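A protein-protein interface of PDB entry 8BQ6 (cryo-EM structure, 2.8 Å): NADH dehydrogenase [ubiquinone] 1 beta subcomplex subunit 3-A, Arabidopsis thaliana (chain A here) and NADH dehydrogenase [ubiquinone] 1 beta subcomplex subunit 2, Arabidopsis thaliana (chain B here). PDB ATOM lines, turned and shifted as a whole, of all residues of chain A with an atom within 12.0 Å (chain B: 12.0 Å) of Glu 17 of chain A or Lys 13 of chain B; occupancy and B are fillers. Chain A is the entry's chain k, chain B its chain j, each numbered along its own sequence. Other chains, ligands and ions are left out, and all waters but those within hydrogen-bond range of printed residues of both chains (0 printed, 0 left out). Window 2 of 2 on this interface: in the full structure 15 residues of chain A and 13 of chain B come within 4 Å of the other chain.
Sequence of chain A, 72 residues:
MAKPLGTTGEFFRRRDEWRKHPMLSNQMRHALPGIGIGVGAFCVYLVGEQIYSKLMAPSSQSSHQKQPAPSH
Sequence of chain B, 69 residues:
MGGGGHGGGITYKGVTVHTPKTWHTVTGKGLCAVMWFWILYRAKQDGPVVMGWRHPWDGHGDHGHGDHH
Among the printed residues, merely in contact across the chains: Met 23 of chain A with Ile 10 of chain B (2.8 Å), Met 23 of chain A with Val 17 of chain B (3.1 Å), Trp 18 of chain A with Val 15 of chain B (3.7 Å), Leu 24 of chain A with Val 17 of chain B (3.8 Å), His 21 of chain A with Ile 10 of chain B (3.8 Å), Lys 20 of chain A with Tyr 12 of chain B (3.8 Å) and His 21 of chain A with Val 17 of chain B (3.98 Å).
The backbone carbonyl oxygen of Ile 10 of chain B sits at hydrogen-bond distance from the side-chain hydroxyl of Thr 16 of chain B (3.3 Å).
N of Ile 10 of chain B is in hydrogen-bond range of O of Val 17 of chain B, 2.9 Å away.
Of the 21 printed residues of chain A, 6 touch a printed residue of chain B.
Hydrophobic or aromatic side chains of chain A within 4 Å of the printed part of chain B: Trp 18, His 21, Met 23 and Leu 24.
Hydrophobic or aromatic side chains of chain B that line the printed part of chain A: Ile 10, Tyr 12, Val 15 and Val 17.
Among the printed residues, 10 pairs touch across the chains.
NE2 of His 21 of chain A sits close to N of Tyr 12 of chain B (3.5 Å).
NZ of Lys 13 of chain B is in hydrogen-bond range of O of Glu 17 of chain A, at 3.0 Å.
A ring nitrogen (NE2) of His 21 of chain A is in hydrogen-bond range of the backbone carbonyl oxygen (O) of Val 15 of chain B (3.2 Å).
Glu 10 of chain A touches none of the printed residues of chain B.
Arg 13 of chain A touches none of the printed residues of chain B.
No residue of chain B comes within 4 Å of Arg 14 of chain A.
No residue of chain B comes within 4 Å of Arg 15 of chain A.
No residue of chain B comes within 4 Å of Asp 16 of chain A.
Of the printed residues of chain B, Glu 17 of chain A touches Lys 13 (3.0 Å).
Trp 18 of chain A touches just one residue of chain B: Val 15 (3.7 Å).
Lys 20 of chain A touches just one residue of chain B: Tyr 12 (3.8 Å).
Of the printed residues of chain B, His 21 of chain A touches Ile 10 (3.8 Å), Tyr 12 (3.2 Å), Val 15 (3.2 Å) and Val 17 (3.98 Å).
Of the printed residues of chain B, Met 23 of chain A touches Ile 10 (2.8 Å) and Val 17 (3.1 Å).
Printed residues of chain B within 4 Å of Leu 24 of chain A: Val 17.
Ser 25 of chain A touches none of the printed residues of chain B.
Printed residues of chain A within 4 Å of Ile 10 of chain B: His 21 and Met 23.
No residue of chain A comes within 4 Å of Thr 11 of chain B.
Of chain A, only Lys 20 (3.8 Å) and His 21 (3.2 Å) come within 4 Å of Tyr 12 of chain B.
No residue of chain A comes within 4 Å of Gly 14 of chain B.
Of the printed residues of chain A, Val 17 of chain B touches His 21 (3.98 Å), Met 23 (3.1 Å) and Leu 24 (3.8 Å).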
ATOM      1  N   PRO A   4      34.786  19.370 -28.255  1.00  0.00           N
ATOM      2  CA  PRO A   4      34.431  19.889 -26.925  1.00  0.00           C
ATOM      3  C   PRO A   4      34.779  18.896 -25.805  1.00  0.00           C
ATOM      4  O   PRO A   4      34.213  19.013 -24.731  1.00  0.00           O
ATOM      5  CB  PRO A   4      32.911  20.105 -27.000  1.00  0.00           C
ATOM      6  CG  PRO A   4      32.451  19.065 -27.987  1.00  0.00           C
ATOM      7  CD  PRO A   4      33.581  18.969 -28.991  1.00  0.00           C
ATOM      8  N   GLY A   6      37.915  18.337 -24.204  1.00  0.00           N
ATOM      9  CA  GLY A   6      38.712  18.999 -23.151  1.00  0.00           C
ATOM     10  C   GLY A   6      37.993  20.182 -22.529  1.00  0.00           C
ATOM     11  O   GLY A   6      37.018  20.671 -23.131  1.00  0.00           O
ATOM     12  N   THR A   7      38.466  20.637 -21.365  1.00  0.00           N
ATOM     13  CA  THR A   7      37.805  21.759 -20.644  1.00  0.00           C
ATOM     14  C   THR A   7      37.748  23.004 -21.540  1.00  0.00           C
ATOM     15  O   THR A   7      36.772  23.764 -21.404  1.00  0.00           O
ATOM     16  CB  THR A   7      38.496  22.035 -19.303  1.00  0.00           C
ATOM     17  OG1 THR A   7      39.821  22.509 -19.549  1.00  0.00           O
ATOM     18  CG2 THR A   7      38.547  20.806 -18.422  1.00  0.00           C
ATOM     19  N   THR A   8      38.742  23.197 -22.418  1.00  0.00           N
ATOM     20  CA  THR A   8      38.695  24.330 -23.334  1.00  0.00           C
ATOM     21  C   THR A   8      37.509  24.206 -24.280  1.00  0.00           C
ATOM     22  O   THR A   8      36.728  25.150 -24.443  1.00  0.00           O
ATOM     23  CB  THR A   8      40.001  24.417 -24.124  1.00  0.00           C
ATOM     24  OG1 THR A   8      41.105  24.402 -23.215  1.00  0.00           O
ATOM     25  CG2 THR A   8      40.047  25.711 -24.906  1.00  0.00           C
ATOM     26  N   GLY A   9      37.349  23.037 -24.904  1.00  0.00           N
ATOM     27  CA  GLY A   9      36.229  22.833 -25.806  1.00  0.00           C
ATOM     28  C   GLY A   9      34.885  22.849 -25.105  1.00  0.00           C
ATOM     29  O   GLY A   9      33.905  23.360 -25.652  1.00  0.00           O
ATOM     30  N   GLU A  10      34.819  22.296 -23.891  1.00  0.00           N
ATOM     31  CA  GLU A  10      33.548  22.219 -23.175  1.00  0.00           C
ATOM     32  C   GLU A  10      33.048  23.603 -22.793  1.00  0.00           C
ATOM     33  O   GLU A  10      31.836  23.850 -22.759  1.00  0.00           O
ATOM     34  CB  GLU A  10      33.699  21.340 -21.932  1.00  0.00           C
ATOM     35  CG  GLU A  10      32.465  21.274 -21.044  1.00  0.00           C
ATOM     36  CD  GLU A  10      31.212  20.891 -21.809  1.00  0.00           C
ATOM     37  OE1 GLU A  10      31.273  19.925 -22.600  1.00  0.00           O
ATOM     38  OE2 GLU A  10      30.165  21.545 -21.607  1.00  0.00           O
ATOM     39  N   PHE A  11      33.972  24.515 -22.488  1.00  0.00           N
ATOM     40  CA  PHE A  11      33.591  25.885 -22.171  1.00  0.00           C
ATOM     41  C   PHE A  11      32.878  26.546 -23.342  1.00  0.00           C
ATOM     42  O   PHE A  11      31.783  27.098 -23.183  1.00  0.00           O
ATOM     43  CB  PHE A  11      34.836  26.687 -21.804  1.00  0.00           C
ATOM     44  CG  PHE A  11      34.544  28.047 -21.252  1.00  0.00           C
ATOM     45  CD1 PHE A  11      33.263  28.409 -20.878  1.00  0.00           C
ATOM     46  CD2 PHE A  11      35.547  28.989 -21.172  1.00  0.00           C
ATOM     47  CE1 PHE A  11      33.003  29.667 -20.392  1.00  0.00           C
ATOM     48  CE2 PHE A  11      35.291  30.250 -20.687  1.00  0.00           C
ATOM     49  CZ  PHE A  11      34.018  30.590 -20.298  1.00  0.00           C
ATOM     50  N   PHE A  12      33.485  26.495 -24.526  1.00  0.00           N
ATOM     51  CA  PHE A  12      32.978  27.279 -25.643  1.00  0.00           C
ATOM     52  C   PHE A  12      31.657  26.731 -26.166  1.00  0.00           C
ATOM     53  O   PHE A  12      30.792  27.511 -26.579  1.00  0.00           O
ATOM     54  CB  PHE A  12      34.049  27.349 -26.729  1.00  0.00           C
ATOM     55  CG  PHE A  12      35.207  28.232 -26.357  1.00  0.00           C
ATOM     56  CD1 PHE A  12      34.983  29.509 -25.871  1.00  0.00           C
ATOM     57  CD2 PHE A  12      36.510  27.775 -26.442  1.00  0.00           C
ATOM     58  CE1 PHE A  12      36.034  30.326 -25.512  1.00  0.00           C
ATOM     59  CE2 PHE A  12      37.566  28.586 -26.080  1.00  0.00           C
ATOM     60  CZ  PHE A  12      37.327  29.864 -25.612  1.00  0.00           C
ATOM     61  N   ARG A  13      31.464  25.411 -26.133  1.00  0.00           N
ATOM     62  CA  ARG A  13      30.149  24.872 -26.468  1.00  0.00           C
ATOM     63  C   ARG A  13      29.101  25.295 -25.451  1.00  0.00           C
ATOM     64  O   ARG A  13      27.942  25.533 -25.810  1.00  0.00           O
ATOM     65  CB  ARG A  13      30.187  23.352 -26.569  1.00  0.00           C
ATOM     66  CG  ARG A  13      29.232  22.833 -27.620  1.00  0.00           C
ATOM     67  CD  ARG A  13      28.730  21.452 -27.283  1.00  0.00           C
ATOM     68  NE  ARG A  13      27.391  21.477 -26.706  1.00  0.00           N
ATOM     69  CZ  ARG A  13      27.051  20.863 -25.581  1.00  0.00           C
ATOM     70  NH1 ARG A  13      27.937  20.182 -24.870  1.00  0.00           N
ATOM     71  NH2 ARG A  13      25.791  20.929 -25.160  1.00  0.00           N
ATOM     72  N   ARG A  14      29.478  25.364 -24.176  1.00  0.00           N
ATOM     73  CA  ARG A  14      28.536  25.828 -23.166  1.00  0.00           C
ATOM     74  C   ARG A  14      28.127  27.273 -23.421  1.00  0.00           C
ATOM     75  O   ARG A  14      26.962  27.637 -23.239  1.00  0.00           O
ATOM     76  CB  ARG A  14      29.139  25.681 -21.774  1.00  0.00           C
ATOM     77  CG  ARG A  14      28.109  25.361 -20.722  1.00  0.00           C
ATOM     78  CD  ARG A  14      27.877  23.862 -20.619  1.00  0.00           C
ATOM     79  NE  ARG A  14      29.056  23.158 -20.126  1.00  0.00           N
ATOM     80  CZ  ARG A  14      29.562  23.300 -18.908  1.00  0.00           C
ATOM     81  NH1 ARG A  14      29.022  24.124 -18.025  1.00  0.00           N
ATOM     82  NH2 ARG A  14      30.637  22.596 -18.565  1.00  0.00           N
ATOM     83  N   ARG A  15      29.074  28.113 -23.840  1.00  0.00           N
ATOM     84  CA  ARG A  15      28.752  29.499 -24.155  1.00  0.00           C
ATOM     85  C   ARG A  15      28.020  29.648 -25.480  1.00  0.00           C
ATOM     86  O   ARG A  15      27.353  30.665 -25.693  1.00  0.00           O
ATOM     87  CB  ARG A  15      30.022  30.337 -24.182  1.00  0.00           C
ATOM     88  CG  ARG A  15      30.776  30.337 -22.878  1.00  0.00           C
ATOM     89  CD  ARG A  15      29.991  31.035 -21.775  1.00  0.00           C
ATOM     90  NE  ARG A  15      29.327  32.247 -22.239  1.00  0.00           N
ATOM     91  CZ  ARG A  15      28.212  32.739 -21.715  1.00  0.00           C
ATOM     92  NH1 ARG A  15      27.646  32.188 -20.653  1.00  0.00           N
ATOM     93  NH2 ARG A  15      27.656  33.816 -22.263  1.00  0.00           N
ATOM     94  N   ASP A  16      28.147  28.674 -26.381  1.00  0.00           N
ATOM     95  CA  ASP A  16      27.483  28.696 -27.676  1.00  0.00           C
ATOM     96  C   ASP A  16      26.090  28.115 -27.610  1.00  0.00           C
ATOM     97  O   ASP A  16      25.501  27.789 -28.648  1.00  0.00           O
ATOM     98  CB  ASP A  16      28.310  27.929 -28.700  1.00  0.00           C
ATOM     99  CG  ASP A  16      29.433  28.753 -29.254  1.00  0.00           C
ATOM    100  OD1 ASP A  16      29.183  29.926 -29.592  1.00  0.00           O
ATOM    101  OD2 ASP A  16      30.566  28.239 -29.333  1.00  0.00           O
ATOM    102  N   GLU A  17      25.559  27.969 -26.404  1.00  0.00           N
ATOM    103  CA  GLU A  17      24.317  27.236 -26.232  1.00  0.00           C
ATOM    104  C   GLU A  17      23.117  28.058 -26.686  1.00  0.00           C
ATOM    105  O   GLU A  17      22.035  27.500 -26.896  1.00  0.00           O
ATOM    106  CB  GLU A  17      24.248  26.754 -24.772  1.00  0.00           C
ATOM    107  CG  GLU A  17      25.274  25.713 -24.375  1.00  0.00           C
ATOM    108  CD  GLU A  17      25.200  25.349 -22.955  1.00  0.00           C
ATOM    109  OE1 GLU A  17      24.473  26.047 -22.232  1.00  0.00           O
ATOM    110  OE2 GLU A  17      25.918  24.394 -22.555  1.00  0.00           O
ATOM    111  N   TRP A  18      23.293  29.371 -26.882  1.00  0.00           N
ATOM    112  CA  TRP A  18      22.245  30.169 -27.517  1.00  0.00           C
ATOM    113  C   TRP A  18      22.179  29.950 -29.025  1.00  0.00           C
ATOM    114  O   TRP A  18      21.164  30.289 -29.642  1.00  0.00           O
ATOM    115  CB  TRP A  18      22.438  31.666 -27.237  1.00  0.00           C
ATOM    116  CG  TRP A  18      23.662  32.270 -27.871  1.00  0.00           C
ATOM    117  CD1 TRP A  18      24.887  32.440 -27.292  1.00  0.00           C
ATOM    118  CD2 TRP A  18      23.781  32.770 -29.208  1.00  0.00           C
ATOM    119  NE1 TRP A  18      25.757  33.017 -28.183  1.00  0.00           N
ATOM    120  CE2 TRP A  18      25.101  33.230 -29.367  1.00  0.00           C
ATOM    121  CE3 TRP A  18      22.897  32.875 -30.284  1.00  0.00           C
ATOM    122  CZ2 TRP A  18      25.558  33.784 -30.557  1.00  0.00           C
ATOM    123  CZ3 TRP A  18      23.353  33.424 -31.464  1.00  0.00           C
ATOM    124  CH2 TRP A  18      24.669  33.871 -31.592  1.00  0.00           C
ATOM    125  N   ARG A  19      23.229  29.398 -29.638  1.00  0.00           N
ATOM    126  CA  ARG A  19      23.229  29.205 -31.087  1.00  0.00           C
ATOM    127  C   ARG A  19      22.270  28.114 -31.541  1.00  0.00           C
ATOM    128  O   ARG A  19      22.144  27.888 -32.750  1.00  0.00           O
ATOM    129  CB  ARG A  19      24.641  28.895 -31.582  1.00  0.00           C
ATOM    130  CG  ARG A  19      25.488  30.138 -31.768  1.00  0.00           C
ATOM    131  CD  ARG A  19      26.932  29.808 -32.049  1.00  0.00           C
ATOM    132  NE  ARG A  19      27.826  30.720 -31.349  1.00  0.00           N
ATOM    133  CZ  ARG A  19      28.255  31.872 -31.845  1.00  0.00           C
ATOM    134  NH1 ARG A  19      27.862  32.301 -33.033  1.00  0.00           N
ATOM    135  NH2 ARG A  19      29.094  32.613 -31.130  1.00  0.00           N
ATOM    136  N   LYS A  20      21.600  27.436 -30.613  1.00  0.00           N
ATOM    137  CA  LYS A  20      20.522  26.512 -30.938  1.00  0.00           C
ATOM    138  C   LYS A  20      19.184  27.214 -31.070  1.00  0.00           C
ATOM    139  O   LYS A  20      18.138  26.578 -30.893  1.00  0.00           O
ATOM    140  CB  LYS A  20      20.434  25.407 -29.884  1.00  0.00           C
ATOM    141  CG  LYS A  20      21.748  24.693 -29.629  1.00  0.00           C
ATOM    142  CD  LYS A  20      22.448  24.355 -30.937  1.00  0.00           C
ATOM    143  CE  LYS A  20      23.637  23.444 -30.710  1.00  0.00           C
ATOM    144  NZ  LYS A  20      23.634  22.297 -31.660  1.00  0.00           N
ATOM    145  N   HIS A  21      19.211  28.506 -31.367  1.00  0.00           N
ATOM    146  CA  HIS A  21      17.992  29.281 -31.514  1.00  0.00           C
ATOM    147  C   HIS A  21      17.092  28.630 -32.562  1.00  0.00           C
ATOM    148  O   HIS A  21      17.594  28.071 -33.545  1.00  0.00           O
ATOM    149  CB  HIS A  21      18.344  30.714 -31.922  1.00  0.00           C
ATOM    150  CG  HIS A  21      17.492  31.762 -31.279  1.00  0.00           C
ATOM    151  ND1 HIS A  21      16.193  32.009 -31.665  1.00  0.00           N
ATOM    152  CD2 HIS A  21      17.755  32.624 -30.269  1.00  0.00           C
ATOM    153  CE1 HIS A  21      15.693  32.982 -30.925  1.00  0.00           C
ATOM    154  NE2 HIS A  21      16.621  33.373 -30.070  1.00  0.00           N
ATOM    155  N   PRO A  22      15.773  28.633 -32.362  1.00  0.00           N
ATOM    156  CA  PRO A  22      14.889  27.989 -33.348  1.00  0.00           C
ATOM    157  C   PRO A  22      15.067  28.507 -34.764  1.00  0.00           C
ATOM    158  O   PRO A  22      15.259  27.711 -35.692  1.00  0.00           O
ATOM    159  CB  PRO A  22      13.490  28.292 -32.801  1.00  0.00           C
ATOM    160  CG  PRO A  22      13.691  28.430 -31.334  1.00  0.00           C
ATOM    161  CD  PRO A  22      15.050  29.037 -31.145  1.00  0.00           C
ATOM    162  N   MET A  23      15.025  29.823 -34.958  1.00  0.00           N
ATOM    163  CA  MET A  23      15.076  30.413 -36.287  1.00  0.00           C
ATOM    164  C   MET A  23      16.472  30.881 -36.676  1.00  0.00           C
ATOM    165  O   MET A  23      16.627  31.578 -37.684  1.00  0.00           O
ATOM    166  CB  MET A  23      14.072  31.563 -36.383  1.00  0.00           C
ATOM    167  CG  MET A  23      14.419  32.756 -35.539  1.00  0.00           C
ATOM    168  SD  MET A  23      13.017  33.876 -35.424  1.00  0.00           S
ATOM    169  CE  MET A  23      12.168  33.195 -34.006  1.00  0.00           C
ATOM    170  N   LEU A  24      17.490  30.513 -35.902  1.00  0.00           N
ATOM    171  CA  LEU A  24      18.872  30.702 -36.310  1.00  0.00           C
ATOM    172  C   LEU A  24      19.515  29.415 -36.805  1.00  0.00           C
ATOM    173  O   LEU A  24      20.525  29.474 -37.512  1.00  0.00           O
ATOM    174  CB  LEU A  24      19.697  31.268 -35.151  1.00  0.00           C
ATOM    175  CG  LEU A  24      19.469  32.734 -34.780  1.00  0.00           C
ATOM    176  CD1 LEU A  24      20.699  33.292 -34.086  1.00  0.00           C
ATOM    177  CD2 LEU A  24      19.103  33.573 -35.999  1.00  0.00           C
ATOM    178  N   SER A  25      18.956  28.262 -36.458  1.00  0.00           N
ATOM    179  CA  SER A  25      19.495  26.980 -36.877  1.00  0.00           C
ATOM    180  C   SER A  25      18.583  26.351 -37.919  1.00  0.00           C
ATOM    181  O   SER A  25      17.478  26.833 -38.190  1.00  0.00           O
ATOM    182  CB  SER A  25      19.672  26.038 -35.682  1.00  0.00           C
ATOM    183  OG  SER A  25      20.646  26.543 -34.788  1.00  0.00           O
ATOM    184  N   GLY B   9       9.650  39.891 -31.343  1.00  0.00           N
ATOM    185  CA  GLY B   9      10.336  38.664 -31.700  1.00  0.00           C
ATOM    186  C   GLY B   9      10.293  37.621 -30.602  1.00  0.00           C
ATOM    187  O   GLY B   9       9.453  37.687 -29.706  1.00  0.00           O
ATOM    188  N   ILE B  10      11.209  36.658 -30.673  1.00  0.00           N
ATOM    189  CA  ILE B  10      11.318  35.574 -29.703  1.00  0.00           C
ATOM    190  C   ILE B  10      12.667  35.673 -29.011  1.00  0.00           C
ATOM    191  O   ILE B  10      13.693  35.899 -29.663  1.00  0.00           O
ATOM    192  CB  ILE B  10      11.142  34.199 -30.371  1.00  0.00           C
ATOM    193  CG1 ILE B  10       9.796  34.134 -31.090  1.00  0.00           C
ATOM    194  CG2 ILE B  10      11.311  33.065 -29.357  1.00  0.00           C
ATOM    195  CD1 ILE B  10       9.910  33.931 -32.567  1.00  0.00           C
ATOM    196  N   THR B  11      12.668  35.514 -27.692  1.00  0.00           N
ATOM    197  CA  THR B  11      13.898  35.511 -26.915  1.00  0.00           C
ATOM    198  C   THR B  11      14.225  34.087 -26.507  1.00  0.00           C
ATOM    199  O   THR B  11      13.396  33.392 -25.910  1.00  0.00           O
ATOM    200  CB  THR B  11      13.800  36.405 -25.681  1.00  0.00           C
ATOM    201  OG1 THR B  11      14.127  37.750 -26.048  1.00  0.00           O
ATOM    202  CG2 THR B  11      14.776  35.938 -24.606  1.00  0.00           C
ATOM    203  N   TYR B  12      15.437  33.665 -26.833  1.00  0.00           N
ATOM    204  CA  TYR B  12      15.990  32.402 -26.378  1.00  0.00           C
ATOM    205  C   TYR B  12      17.295  32.751 -25.675  1.00  0.00           C
ATOM    206  O   TYR B  12      18.320  32.962 -26.331  1.00  0.00           O
ATOM    207  CB  TYR B  12      16.176  31.449 -27.559  1.00  0.00           C
ATOM    208  CG  TYR B  12      16.255  29.975 -27.243  1.00  0.00           C
ATOM    209  CD1 TYR B  12      17.338  29.224 -27.657  1.00  0.00           C
ATOM    210  CD2 TYR B  12      15.247  29.336 -26.530  1.00  0.00           C
ATOM    211  CE1 TYR B  12      17.409  27.879 -27.403  1.00  0.00           C
ATOM    212  CE2 TYR B  12      15.324  27.985 -26.247  1.00  0.00           C
ATOM    213  CZ  TYR B  12      16.411  27.263 -26.681  1.00  0.00           C
ATOM    214  OH  TYR B  12      16.503  25.918 -26.411  1.00  0.00           O
ATOM    215  N   LYS B  13      17.215  32.895 -24.353  1.00  0.00           N
ATOM    216  CA  LYS B  13      18.350  33.017 -23.421  1.00  0.00           C
ATOM    217  C   LYS B  13      19.324  34.132 -23.800  1.00  0.00           C
ATOM    218  O   LYS B  13      20.436  33.899 -24.273  1.00  0.00           O
ATOM    219  CB  LYS B  13      19.077  31.684 -23.224  1.00  0.00           C
ATOM    220  CG  LYS B  13      19.591  30.956 -24.434  1.00  0.00           C
ATOM    221  CD  LYS B  13      20.060  29.672 -24.022  1.00  0.00           C
ATOM    222  CE  LYS B  13      19.076  28.550 -24.232  1.00  0.00           C
ATOM    223  NZ  LYS B  13      19.478  27.812 -25.454  1.00  0.00           N
ATOM    224  N   GLY B  14      18.867  35.367 -23.603  1.00  0.00           N
ATOM    225  CA  GLY B  14      19.720  36.526 -23.776  1.00  0.00           C
ATOM    226  C   GLY B  14      19.619  37.073 -25.179  1.00  0.00           C
ATOM    227  O   GLY B  14      19.309  38.250 -25.385  1.00  0.00           O
ATOM    228  N   VAL B  15      19.855  36.209 -26.154  1.00  0.00           N
ATOM    229  CA  VAL B  15      19.844  36.614 -27.553  1.00  0.00           C
ATOM    230  C   VAL B  15      18.410  36.582 -28.063  1.00  0.00           C
ATOM    231  O   VAL B  15      17.739  35.545 -28.008  1.00  0.00           O
ATOM    232  CB  VAL B  15      20.760  35.701 -28.381  1.00  0.00           C
ATOM    233  CG1 VAL B  15      20.709  36.085 -29.848  1.00  0.00           C
ATOM    234  CG2 VAL B  15      22.186  35.761 -27.840  1.00  0.00           C
ATOM    235  N   THR B  16      17.939  37.722 -28.557  1.00  0.00           N
ATOM    236  CA  THR B  16      16.583  37.871 -29.065  1.00  0.00           C
ATOM    237  C   THR B  16      16.635  38.003 -30.581  1.00  0.00           C
ATOM    238  O   THR B  16      17.530  38.661 -31.122  1.00  0.00           O
ATOM    239  CB  THR B  16      15.892  39.081 -28.415  1.00  0.00           C
ATOM    240  OG1 THR B  16      14.469  38.934 -28.500  1.00  0.00           O
ATOM    241  CG2 THR B  16      16.313  40.405 -29.057  1.00  0.00           C
ATOM    242  N   VAL B  17      15.712  37.340 -31.269  1.00  0.00           N
ATOM    243  CA  VAL B  17      15.594  37.445 -32.719  1.00  0.00           C
ATOM    244  C   VAL B  17      14.243  38.059 -33.037  1.00  0.00           C
ATOM    245  O   VAL B  17      13.206  37.574 -32.569  1.00  0.00           O
ATOM    246  CB  VAL B  17      15.743  36.086 -33.420  1.00  0.00           C
ATOM    247  CG1 VAL B  17      15.042  36.126 -34.771  1.00  0.00           C
ATOM    248  CG2 VAL B  17      17.203  35.739 -33.597  1.00  0.00           C
ATOM    249  N   HIS B  18      14.255  39.123 -33.829  1.00  0.00           N
ATOM    250  CA  HIS B  18      13.028  39.761 -34.271  1.00  0.00           C
ATOM    251  C   HIS B  18      12.529  39.097 -35.545  1.00  0.00           C
ATOM    252  O   HIS B  18      13.308  38.807 -36.456  1.00  0.00           O
ATOM    253  CB  HIS B  18      13.256  41.252 -34.508  1.00  0.00           C
ATOM    254  CG  HIS B  18      14.140  41.890 -33.485  1.00  0.00           C
ATOM    255  ND1 HIS B  18      15.498  42.037 -33.665  1.00  0.00           N
ATOM    256  CD2 HIS B  18      13.862  42.411 -32.267  1.00  0.00           C
ATOM    257  CE1 HIS B  18      16.018  42.627 -32.604  1.00  0.00           C
ATOM    258  NE2 HIS B  18      15.046  42.865 -31.742  1.00  0.00           N
